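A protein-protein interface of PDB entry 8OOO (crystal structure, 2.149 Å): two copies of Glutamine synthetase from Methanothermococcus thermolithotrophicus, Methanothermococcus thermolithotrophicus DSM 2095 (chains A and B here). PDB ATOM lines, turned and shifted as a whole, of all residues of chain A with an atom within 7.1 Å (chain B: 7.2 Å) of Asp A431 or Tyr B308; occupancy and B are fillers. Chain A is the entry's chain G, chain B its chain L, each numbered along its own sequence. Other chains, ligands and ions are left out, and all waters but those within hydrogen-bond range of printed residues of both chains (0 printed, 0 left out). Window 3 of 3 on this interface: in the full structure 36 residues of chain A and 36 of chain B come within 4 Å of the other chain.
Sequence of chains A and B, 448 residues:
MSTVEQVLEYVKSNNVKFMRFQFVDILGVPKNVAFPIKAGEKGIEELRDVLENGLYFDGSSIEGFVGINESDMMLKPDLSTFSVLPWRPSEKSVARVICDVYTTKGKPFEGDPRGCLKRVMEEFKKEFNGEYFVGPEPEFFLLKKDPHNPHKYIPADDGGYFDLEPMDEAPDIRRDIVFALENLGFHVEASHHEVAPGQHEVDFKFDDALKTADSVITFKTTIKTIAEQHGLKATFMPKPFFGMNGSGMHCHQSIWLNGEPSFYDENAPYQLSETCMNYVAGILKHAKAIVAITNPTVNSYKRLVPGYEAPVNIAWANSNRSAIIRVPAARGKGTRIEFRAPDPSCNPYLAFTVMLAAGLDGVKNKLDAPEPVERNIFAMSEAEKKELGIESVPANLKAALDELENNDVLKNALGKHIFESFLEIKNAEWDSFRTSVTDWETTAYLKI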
ATOM      1  N   VAL A 298      21.076  15.397  -6.091  1.00  0.00           N
ATOM      2  CA  VAL A 298      22.237  16.226  -6.441  1.00  0.00           C
ATOM      3  C   VAL A 298      22.940  16.669  -5.142  1.00  0.00           C
ATOM      4  O   VAL A 298      24.180  16.639  -5.041  1.00  0.00           O
ATOM      5  CB  VAL A 298      21.798  17.454  -7.264  1.00  0.00           C
ATOM      6  CG1 VAL A 298      22.922  18.504  -7.359  1.00  0.00           C
ATOM      7  CG2 VAL A 298      21.302  17.011  -8.636  1.00  0.00           C
ATOM      8  N   LYS A 398      25.143  12.170 -11.430  1.00  0.00           N
ATOM      9  CA  LYS A 398      25.262  11.576 -12.730  1.00  0.00           C
ATOM     10  C   LYS A 398      26.368  10.525 -12.783  1.00  0.00           C
ATOM     11  O   LYS A 398      26.170   9.480 -13.401  1.00  0.00           O
ATOM     12  CB  LYS A 398      25.506  12.648 -13.780  1.00  0.00           C
ATOM     13  CG  LYS A 398      25.711  12.072 -15.181  1.00  0.00           C
ATOM     14  CD  LYS A 398      24.548  11.219 -15.596  1.00  0.00           C
ATOM     15  CE  LYS A 398      24.517  11.038 -17.079  1.00  0.00           C
ATOM     16  NZ  LYS A 398      23.702   9.856 -17.468  1.00  0.00           N
ATOM     17  N   GLU A 424      15.821   6.915 -15.261  1.00  0.00           N
ATOM     18  CA  GLU A 424      15.131   7.893 -16.086  1.00  0.00           C
ATOM     19  C   GLU A 424      14.775   9.117 -15.270  1.00  0.00           C
ATOM     20  O   GLU A 424      15.005  10.236 -15.731  1.00  0.00           O
ATOM     21  CB  GLU A 424      13.868   7.276 -16.686  1.00  0.00           C
ATOM     22  CG  GLU A 424      13.153   8.203 -17.628  1.00  0.00           C
ATOM     23  CD  GLU A 424      11.963   7.492 -18.239  1.00  0.00           C
ATOM     24  OE1 GLU A 424      11.058   7.074 -17.475  1.00  0.00           O
ATOM     25  OE2 GLU A 424      11.971   7.278 -19.475  1.00  0.00           O
ATOM     26  N   ILE A 425      14.172   8.908 -14.085  1.00  0.00           N
ATOM     27  CA  ILE A 425      13.772  10.021 -13.225  1.00  0.00           C
ATOM     28  C   ILE A 425      15.002  10.828 -12.811  1.00  0.00           C
ATOM     29  O   ILE A 425      14.989  12.055 -12.877  1.00  0.00           O
ATOM     30  CB  ILE A 425      13.002   9.488 -11.966  1.00  0.00           C
ATOM     31  CG1 ILE A 425      11.582   9.039 -12.366  1.00  0.00           C
ATOM     32  CG2 ILE A 425      12.959  10.538 -10.837  1.00  0.00           C
ATOM     33  CD1 ILE A 425      10.922   8.103 -11.392  1.00  0.00           C
ATOM     34  N   LYS A 426      16.068  10.135 -12.381  1.00  0.00           N
ATOM     35  CA  LYS A 426      17.253  10.806 -11.883  1.00  0.00           C
ATOM     36  C   LYS A 426      18.062  11.470 -12.986  1.00  0.00           C
ATOM     37  O   LYS A 426      18.751  12.450 -12.715  1.00  0.00           O
ATOM     38  CB  LYS A 426      18.108   9.841 -11.060  1.00  0.00           C
ATOM     39  CG  LYS A 426      17.367   9.327  -9.847  1.00  0.00           C
ATOM     40  CD  LYS A 426      17.482  10.340  -8.739  1.00  0.00           C
ATOM     41  CE  LYS A 426      16.241  10.450  -7.889  1.00  0.00           C
ATOM     42  NZ  LYS A 426      16.386  11.517  -6.865  1.00  0.00           N
ATOM     43  N   ASN A 427      17.976  10.973 -14.229  1.00  0.00           N
ATOM     44  CA  ASN A 427      18.654  11.644 -15.320  1.00  0.00           C
ATOM     45  C   ASN A 427      17.917  12.947 -15.633  1.00  0.00           C
ATOM     46  O   ASN A 427      18.565  13.925 -15.960  1.00  0.00           O
ATOM     47  CB  ASN A 427      18.766  10.773 -16.559  1.00  0.00           C
ATOM     48  CG  ASN A 427      20.077  10.054 -16.668  1.00  0.00           C
ATOM     49  OD1 ASN A 427      21.144  10.677 -16.770  1.00  0.00           O
ATOM     50  ND2 ASN A 427      20.030   8.728 -16.619  1.00  0.00           N
ATOM     51  N   ALA A 428      16.573  12.981 -15.529  1.00  0.00           N
ATOM     52  CA  ALA A 428      15.826  14.225 -15.743  1.00  0.00           C
ATOM     53  C   ALA A 428      16.103  15.226 -14.600  1.00  0.00           C
ATOM     54  O   ALA A 428      16.180  16.428 -14.823  1.00  0.00           O
ATOM     55  CB  ALA A 428      14.347  13.939 -15.842  1.00  0.00           C
ATOM     56  N   GLU A 429      16.278  14.718 -13.382  1.00  0.00           N
ATOM     57  CA  GLU A 429      16.597  15.545 -12.225  1.00  0.00           C
ATOM     58  C   GLU A 429      17.983  16.160 -12.404  1.00  0.00           C
ATOM     59  O   GLU A 429      18.171  17.343 -12.169  1.00  0.00           O
ATOM     60  CB  GLU A 429      16.558  14.666 -10.977  1.00  0.00           C
ATOM     61  CG  GLU A 429      16.747  15.416  -9.683  1.00  0.00           C
ATOM     62  CD  GLU A 429      16.488  14.531  -8.486  1.00  0.00           C
ATOM     63  OE1 GLU A 429      15.640  13.609  -8.576  1.00  0.00           O
ATOM     64  OE2 GLU A 429      17.170  14.747  -7.462  1.00  0.00           O
ATOM     65  N   TRP A 430      18.951  15.361 -12.862  1.00  0.00           N
ATOM     66  CA  TRP A 430      20.308  15.850 -13.157  1.00  0.00           C
ATOM     67  C   TRP A 430      20.267  16.914 -14.270  1.00  0.00           C
ATOM     68  O   TRP A 430      20.949  17.925 -14.166  1.00  0.00           O
ATOM     69  CB  TRP A 430      21.206  14.668 -13.591  1.00  0.00           C
ATOM     70  CG  TRP A 430      22.613  15.064 -13.941  1.00  0.00           C
ATOM     71  CD1 TRP A 430      23.187  15.071 -15.182  1.00  0.00           C
ATOM     72  CD2 TRP A 430      23.601  15.593 -13.040  1.00  0.00           C
ATOM     73  NE1 TRP A 430      24.486  15.528 -15.100  1.00  0.00           N
ATOM     74  CE2 TRP A 430      24.752  15.883 -13.803  1.00  0.00           C
ATOM     75  CE3 TRP A 430      23.623  15.845 -11.665  1.00  0.00           C
ATOM     76  CZ2 TRP A 430      25.925  16.344 -13.219  1.00  0.00           C
ATOM     77  CZ3 TRP A 430      24.766  16.368 -11.114  1.00  0.00           C
ATOM     78  CH2 TRP A 430      25.922  16.548 -11.878  1.00  0.00           C
ATOM     79  N   ASP A 431      19.497  16.660 -15.350  1.00  0.00           N
ATOM     80  CA  ASP A 431      19.368  17.611 -16.463  1.00  0.00           C
ATOM     81  C   ASP A 431      18.810  18.947 -15.993  1.00  0.00           C
ATOM     82  O   ASP A 431      19.182  20.014 -16.502  1.00  0.00           O
ATOM     83  CB  ASP A 431      18.452  17.057 -17.557  1.00  0.00           C
ATOM     84  CG  ASP A 431      19.049  15.912 -18.360  1.00  0.00           C
ATOM     85  OD1 ASP A 431      20.279  15.691 -18.261  1.00  0.00           O
ATOM     86  OD2 ASP A 431      18.285  15.236 -19.086  1.00  0.00           O
ATOM     87  N   SER A 432      17.876  18.894 -15.063  1.00  0.00           N
ATOM     88  CA  SER A 432      17.273  20.104 -14.528  1.00  0.00           C
ATOM     89  C   SER A 432      18.330  20.920 -13.781  1.00  0.00           C
ATOM     90  O   SER A 432      18.463  22.115 -14.008  1.00  0.00           O
ATOM     91  CB  SER A 432      16.117  19.743 -13.604  1.00  0.00           C
ATOM     92  OG  SER A 432      15.701  20.912 -12.927  1.00  0.00           O
ATOM     93  N   PHE A 433      19.112  20.257 -12.941  1.00  0.00           N
ATOM     94  CA  PHE A 433      20.157  20.904 -12.186  1.00  0.00           C
ATOM     95  C   PHE A 433      21.253  21.460 -13.113  1.00  0.00           C
ATOM     96  O   PHE A 433      21.660  22.627 -12.966  1.00  0.00           O
ATOM     97  CB  PHE A 433      20.746  19.931 -11.146  1.00  0.00           C
ATOM     98  CG  PHE A 433      21.998  20.455 -10.456  1.00  0.00           C
ATOM     99  CD1 PHE A 433      21.943  21.579  -9.643  1.00  0.00           C
ATOM    100  CD2 PHE A 433      23.214  19.813 -10.614  1.00  0.00           C
ATOM    101  CE1 PHE A 433      23.085  22.029  -8.974  1.00  0.00           C
ATOM    102  CE2 PHE A 433      24.364  20.299  -9.982  1.00  0.00           C
ATOM    103  CZ  PHE A 433      24.303  21.412  -9.184  1.00  0.00           C
ATOM    104  N   ARG A 434      21.738  20.650 -14.065  1.00  0.00           N
ATOM    105  CA  ARG A 434      22.858  21.059 -14.895  1.00  0.00           C
ATOM    106  C   ARG A 434      22.521  22.155 -15.902  1.00  0.00           C
ATOM    107  O   ARG A 434      23.445  22.820 -16.374  1.00  0.00           O
ATOM    108  CB  ARG A 434      23.510  19.847 -15.568  1.00  0.00           C
ATOM    109  CG  ARG A 434      22.836  19.386 -16.878  1.00  0.00           C
ATOM    110  CD  ARG A 434      23.276  17.976 -17.231  1.00  0.00           C
ATOM    111  NE  ARG A 434      22.520  17.449 -18.374  1.00  0.00           N
ATOM    112  CZ  ARG A 434      22.822  17.658 -19.655  1.00  0.00           C
ATOM    113  NH1 ARG A 434      23.870  18.408 -19.989  1.00  0.00           N
ATOM    114  NH2 ARG A 434      22.068  17.133 -20.611  1.00  0.00           N
ATOM    115  N   THR A 435      21.234  22.393 -16.201  1.00  0.00           N
ATOM    116  CA  THR A 435      20.844  23.488 -17.106  1.00  0.00           C
ATOM    117  C   THR A 435      20.463  24.759 -16.357  1.00  0.00           C
ATOM    118  O   THR A 435      20.316  25.801 -16.989  1.00  0.00           O
ATOM    119  CB  THR A 435      19.675  23.068 -17.994  1.00  0.00           C
ATOM    120  OG1 THR A 435      18.583  22.646 -17.186  1.00  0.00           O
ATOM    121  CG2 THR A 435      20.048  21.995 -18.982  1.00  0.00           C
ATOM    122  N   SER A 436      20.304  24.700 -15.032  1.00  0.00           N
ATOM    123  CA  SER A 436      19.938  25.879 -14.258  1.00  0.00           C
ATOM    124  C   SER A 436      21.106  26.814 -14.100  1.00  0.00           C
ATOM    125  O   SER A 436      22.246  26.376 -14.138  1.00  0.00           O
ATOM    126  CB  SER A 436      19.434  25.454 -12.881  1.00  0.00           C
ATOM    127  OG  SER A 436      20.536  25.090 -12.057  1.00  0.00           O
ATOM    128  N   PHE B 242      18.536  31.801 -16.839  1.00  0.00           N
ATOM    129  CA  PHE B 242      17.986  30.549 -17.335  1.00  0.00           C
ATOM    130  C   PHE B 242      16.740  30.908 -18.177  1.00  0.00           C
ATOM    131  O   PHE B 242      16.039  31.840 -17.836  1.00  0.00           O
ATOM    132  CB  PHE B 242      17.589  29.638 -16.166  1.00  0.00           C
ATOM    133  CG  PHE B 242      16.817  28.420 -16.619  1.00  0.00           C
ATOM    134  CD1 PHE B 242      17.474  27.331 -17.167  1.00  0.00           C
ATOM    135  CD2 PHE B 242      15.426  28.420 -16.625  1.00  0.00           C
ATOM    136  CE1 PHE B 242      16.758  26.243 -17.678  1.00  0.00           C
ATOM    137  CE2 PHE B 242      14.718  27.371 -17.198  1.00  0.00           C
ATOM    138  CZ  PHE B 242      15.391  26.270 -17.684  1.00  0.00           C
ATOM    139  N   ARG B 303      25.332  27.399 -21.209  1.00  0.00           N
ATOM    140  CA  ARG B 303      25.055  27.797 -22.577  1.00  0.00           C
ATOM    141  C   ARG B 303      25.532  26.608 -23.474  1.00  0.00           C
ATOM    142  O   ARG B 303      24.790  26.110 -24.317  1.00  0.00           O
ATOM    143  CB  ARG B 303      25.809  29.097 -22.915  1.00  0.00           C
ATOM    144  CG  ARG B 303      25.989  29.315 -24.402  1.00  0.00           C
ATOM    145  CD  ARG B 303      26.727  30.585 -24.749  1.00  0.00           C
ATOM    146  NE  ARG B 303      27.005  30.622 -26.189  1.00  0.00           N
ATOM    147  CZ  ARG B 303      28.042  30.031 -26.790  1.00  0.00           C
ATOM    148  NH1 ARG B 303      28.947  29.367 -26.073  1.00  0.00           N
ATOM    149  NH2 ARG B 303      28.184  30.101 -28.106  1.00  0.00           N
ATOM    150  N   VAL B 305      25.637  23.430 -23.435  1.00  0.00           N
ATOM    151  CA  VAL B 305      25.089  22.322 -22.659  1.00  0.00           C
ATOM    152  C   VAL B 305      24.647  21.140 -23.538  1.00  0.00           C
ATOM    153  O   VAL B 305      23.607  21.208 -24.225  1.00  0.00           O
ATOM    154  CB  VAL B 305      23.975  22.844 -21.682  1.00  0.00           C
ATOM    155  CG1 VAL B 305      22.853  23.557 -22.415  1.00  0.00           C
ATOM    156  CG2 VAL B 305      23.442  21.727 -20.803  1.00  0.00           C
ATOM    157  N   PRO B 306      25.457  20.036 -23.539  1.00  0.00           N
ATOM    158  CA  PRO B 306      25.078  18.862 -24.335  1.00  0.00           C
ATOM    159  C   PRO B 306      23.669  18.354 -24.043  1.00  0.00           C
ATOM    160  O   PRO B 306      23.219  18.360 -22.896  1.00  0.00           O
ATOM    161  CB  PRO B 306      26.138  17.823 -23.969  1.00  0.00           C
ATOM    162  CG  PRO B 306      27.316  18.603 -23.554  1.00  0.00           C
ATOM    163  CD  PRO B 306      26.737  19.805 -22.832  1.00  0.00           C
ATOM    164  N   GLY B 307      22.989  17.915 -25.099  1.00  0.00           N
ATOM    165  CA  GLY B 307      21.635  17.416 -25.005  1.00  0.00           C
ATOM    166  C   GLY B 307      20.601  18.471 -25.320  1.00  0.00           C
ATOM    167  O   GLY B 307      19.400  18.180 -25.321  1.00  0.00           O
ATOM    168  N   TYR B 308      21.044  19.719 -25.564  1.00  0.00           N
ATOM    169  CA  TYR B 308      20.120  20.815 -25.856  1.00  0.00           C
ATOM    170  C   TYR B 308      20.535  21.572 -27.121  1.00  0.00           C
ATOM    171  O   TYR B 308      21.509  21.203 -27.775  1.00  0.00           O
ATOM    172  CB  TYR B 308      20.046  21.737 -24.639  1.00  0.00           C
ATOM    173  CG  TYR B 308      19.516  21.026 -23.411  1.00  0.00           C
ATOM    174  CD1 TYR B 308      20.350  20.235 -22.625  1.00  0.00           C
ATOM    175  CD2 TYR B 308      18.166  21.039 -23.110  1.00  0.00           C
ATOM    176  CE1 TYR B 308      19.851  19.497 -21.555  1.00  0.00           C
ATOM    177  CE2 TYR B 308      17.655  20.304 -22.046  1.00  0.00           C
ATOM    178  CZ  TYR B 308      18.505  19.550 -21.257  1.00  0.00           C
ATOM    179  OH  TYR B 308      17.986  18.890 -20.166  1.00  0.00           O
ATOM    180  N   GLU B 309      19.773  22.615 -27.482  1.00  0.00           N
ATOM    181  CA  GLU B 309      20.095  23.445 -28.643  1.00  0.00           C
ATOM    182  C   GLU B 309      21.269  24.357 -28.278  1.00  0.00           C
ATOM    183  O   GLU B 309      21.067  25.398 -27.691  1.00  0.00           O
ATOM    184  CB  GLU B 309      18.879  24.267 -29.086  1.00  0.00           C
ATOM    185  CG  GLU B 309      17.692  23.392 -29.381  1.00  0.00           C
ATOM    186  CD  GLU B 309      16.646  23.995 -30.299  1.00  0.00           C
ATOM    187  OE1 GLU B 309      15.755  23.232 -30.738  1.00  0.00           O
ATOM    188  OE2 GLU B 309      16.725  25.216 -30.580  1.00  0.00           O
ATOM    189  N   ALA B 310      22.495  23.936 -28.603  1.00  0.00           N
ATOM    190  CA  ALA B 310      23.713  24.674 -28.282  1.00  0.00           C
ATOM    191  C   ALA B 310      24.815  24.303 -29.268  1.00  0.00           C
ATOM    192  O   ALA B 310      24.668  23.298 -29.969  1.00  0.00           O
ATOM    193  CB  ALA B 310      24.140  24.323 -26.868  1.00  0.00           C
ATOM    194  N   PRO B 311      25.922  25.089 -29.378  1.00  0.00           N
ATOM    195  CA  PRO B 311      26.997  24.721 -30.331  1.00  0.00           C
ATOM    196  C   PRO B 311      27.898  23.638 -29.749  1.00  0.00           C
ATOM    197  O   PRO B 311      29.101  23.849 -29.581  1.00  0.00           O
ATOM    198  CB  PRO B 311      27.730  26.049 -30.594  1.00  0.00           C
ATOM    199  CG  PRO B 311      27.317  26.981 -29.458  1.00  0.00           C
ATOM    200  CD  PRO B 311      26.271  26.313 -28.610  1.00  0.00           C
ATOM    201  N   VAL B 312      27.312  22.465 -29.485  1.00  0.00           N
ATOM    202  CA  VAL B 312      27.943  21.325 -28.788  1.00  0.00           C
ATOM    203  C   VAL B 312      28.263  20.141 -29.702  1.00  0.00           C
ATOM    204  O   VAL B 312      29.063  19.280 -29.337  1.00  0.00           O
ATOM    205  CB  VAL B 312      27.043  20.848 -27.601  1.00  0.00           C
ATOM    206  CG1 VAL B 312      26.907  21.946 -26.540  1.00  0.00           C
ATOM    207  CG2 VAL B 312      25.670  20.381 -28.076  1.00  0.00           C
ATOM    208  N   ASN B 313      27.579  20.054 -30.854  1.00  0.00           N
ATOM    209  CA  ASN B 313      27.711  18.947 -31.780  1.00  0.00           C
ATOM    210  C   ASN B 313      28.941  19.113 -32.645  1.00  0.00           C
ATOM    211  O   ASN B 313      29.076  20.104 -33.370  1.00  0.00           O
ATOM    212  CB  ASN B 313      26.433  18.809 -32.595  1.00  0.00           C
ATOM    213  CG  ASN B 313      25.287  18.472 -31.672  1.00  0.00           C
ATOM    214  OD1 ASN B 313      25.262  17.359 -31.101  1.00  0.00           O
ATOM    215  ND2 ASN B 313      24.353  19.430 -31.432  1.00  0.00           N
ATOM    216  N   PHE B 378      19.804  19.619 -34.222  1.00  0.00           N
ATOM    217  CA  PHE B 378      18.942  19.622 -33.034  1.00  0.00           C
ATOM    218  C   PHE B 378      17.678  18.783 -33.233  1.00  0.00           C
ATOM    219  O   PHE B 378      17.028  18.454 -32.240  1.00  0.00           O
ATOM    220  CB  PHE B 378      18.575  21.057 -32.630  1.00  0.00           C
ATOM    221  CG  PHE B 378      19.775  21.956 -32.449  1.00  0.00           C
ATOM    222  CD1 PHE B 378      20.947  21.474 -31.904  1.00  0.00           C
ATOM    223  CD2 PHE B 378      19.722  23.290 -32.780  1.00  0.00           C
ATOM    224  CE1 PHE B 378      22.039  22.302 -31.713  1.00  0.00           C
ATOM    225  CE2 PHE B 378      20.784  24.143 -32.499  1.00  0.00           C
ATOM    226  CZ  PHE B 378      21.949  23.636 -31.985  1.00  0.00           C
ATOM    227  N   LYS B 385      22.608  10.519 -34.197  1.00  0.00           N
ATOM    228  CA  LYS B 385      23.865  11.254 -34.141  1.00  0.00           C
ATOM    229  C   LYS B 385      25.021  10.292 -33.864  1.00  0.00           C
ATOM    230  O   LYS B 385      26.102  10.456 -34.420  1.00  0.00           O
ATOM    231  CB  LYS B 385      23.787  12.320 -33.044  1.00  0.00           C
ATOM    232  CG  LYS B 385      22.824  13.444 -33.376  1.00  0.00           C
ATOM    233  CD  LYS B 385      22.960  14.610 -32.442  1.00  0.00           C
ATOM    234  CE  LYS B 385      22.382  14.316 -31.086  1.00  0.00           C
ATOM    235  NZ  LYS B 385      22.399  15.504 -30.200  1.00  0.00           N
ATOM    236  N   SER B 392      29.570  15.035 -28.910  1.00  0.00           N
ATOM    237  CA  SER B 392      29.375  16.299 -28.218  1.00  0.00           C
ATOM    238  C   SER B 392      30.631  16.691 -27.451  1.00  0.00           C
ATOM    239  O   SER B 392      31.480  15.849 -27.109  1.00  0.00           O
ATOM    240  CB  SER B 392      28.202  16.215 -27.241  1.00  0.00           C
ATOM    241  OG  SER B 392      26.968  16.467 -27.901  1.00  0.00           O
ATOM    242  N   TRP B 440      19.190  26.095  -6.381  1.00  0.00           N
ATOM    243  CA  TRP B 440      18.421  25.056  -7.080  1.00  0.00           C
ATOM    244  C   TRP B 440      18.171  23.891  -6.121  1.00  0.00           C
ATOM    245  O   TRP B 440      17.027  23.416  -6.000  1.00  0.00           O
ATOM    246  CB  TRP B 440      19.147  24.559  -8.351  1.00  0.00           C
ATOM    247  CG  TRP B 440      18.361  23.525  -9.139  1.00  0.00           C
ATOM    248  CD1 TRP B 440      17.587  23.747 -10.238  1.00  0.00           C
ATOM    249  CD2 TRP B 440      18.292  22.104  -8.885  1.00  0.00           C
ATOM    250  NE1 TRP B 440      17.048  22.564 -10.688  1.00  0.00           N
ATOM    251  CE2 TRP B 440      17.409  21.551  -9.835  1.00  0.00           C
ATOM    252  CE3 TRP B 440      18.863  21.254  -7.928  1.00  0.00           C
ATOM    253  CZ2 TRP B 440      17.141  20.174  -9.896  1.00  0.00           C
ATOM    254  CZ3 TRP B 440      18.568  19.900  -7.965  1.00  0.00           C
ATOM    255  CH2 TRP B 440      17.684  19.379  -8.918  1.00  0.00           C
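Of the 15 printed residues of chain B, 5 touch a printed residue of chain A. Hydrophobic or aromatic side chains of chain A within 4 Å of the printed part of chain B: Phe A433. Along chain A the printed residues that touch a printed residue of chain B span positions 429 to 436. Among the printed residues, 11 pairs touch across the chains. Among the printed residues, no Asp or Glu carboxylate lies within 4 Å of a Lys or Arg side-chain nitrogen of the other chain.
Asp A431 touches just one residue of chain B: Tyr B308 (3.2 Å). Of chain A, only Asp A431, Arg A434 and Thr A435 come within 4 Å of Tyr B308. No residue of chain A comes within 4 Å of Gly B307. Of the printed residues of chain A, Phe B242 touches Thr A435 (3.2 Å). Of the printed residues of chain B, Ser A436 touches Trp B440. Printed residues of chain B within 4 Å of Ser A432: Trp B440. Of the printed residues of chain A, Trp B440 touches Glu A429 (3.8 Å), Ser A432 (3.1 Å), Phe A433 (3.5 Å) and Ser A436 (3.6 Å). Of the printed residues of chain A, Val B305 touches Arg A434 (3.4 Å) and Thr A435 (3.9 Å). The nearest residue of chain B that does not touch Asp A431 is Pro B306 (6.1 Å).
No position is printed for both chains. Of the 11 pairs that touch across the chains among the printed residues, none has its exchanged pair printed and touching as well.
NZ of Lys A426 is in salt-bridge range of OE1 of Glu A429, 2.8 Å away. NE of Arg A434 lies within salt-bridge range of OD1 of Asp A431, 2.9 Å away. O of Asp A431 sits at hydrogen-bond distance from OG1 of Thr A435, at 2.8 Å. The side-chain hydroxyl (OG1) of Thr A435 sits at hydrogen-bond distance from the backbone carbonyl oxygen (O) of Ser A432. OG of Ser A436 is in hydrogen-bond range of O of Phe A433 (2.9 Å).
Among the printed residues, pairs that only touch across the chains: Asp A431 with Tyr B308, Thr A435 with Phe B242, Arg A434 with Tyr B308, Arg A434 with Val B305, Phe A433 with Trp B440, Thr A435 with Tyr B308, Ser A436 with Trp B440, Glu A429 with Trp B440 and Thr A435 with Val B305.
The indole nitrogen (NE1) of Trp B440 sits at hydrogen-bond distance from the side-chain hydroxyl (OG) of Ser A432 (3.1 Å). The guanidinium group (NH2) of Arg A434 sits at hydrogen-bond distance from the backbone carbonyl oxygen (O) of Pro B306, 2.8 Å away.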
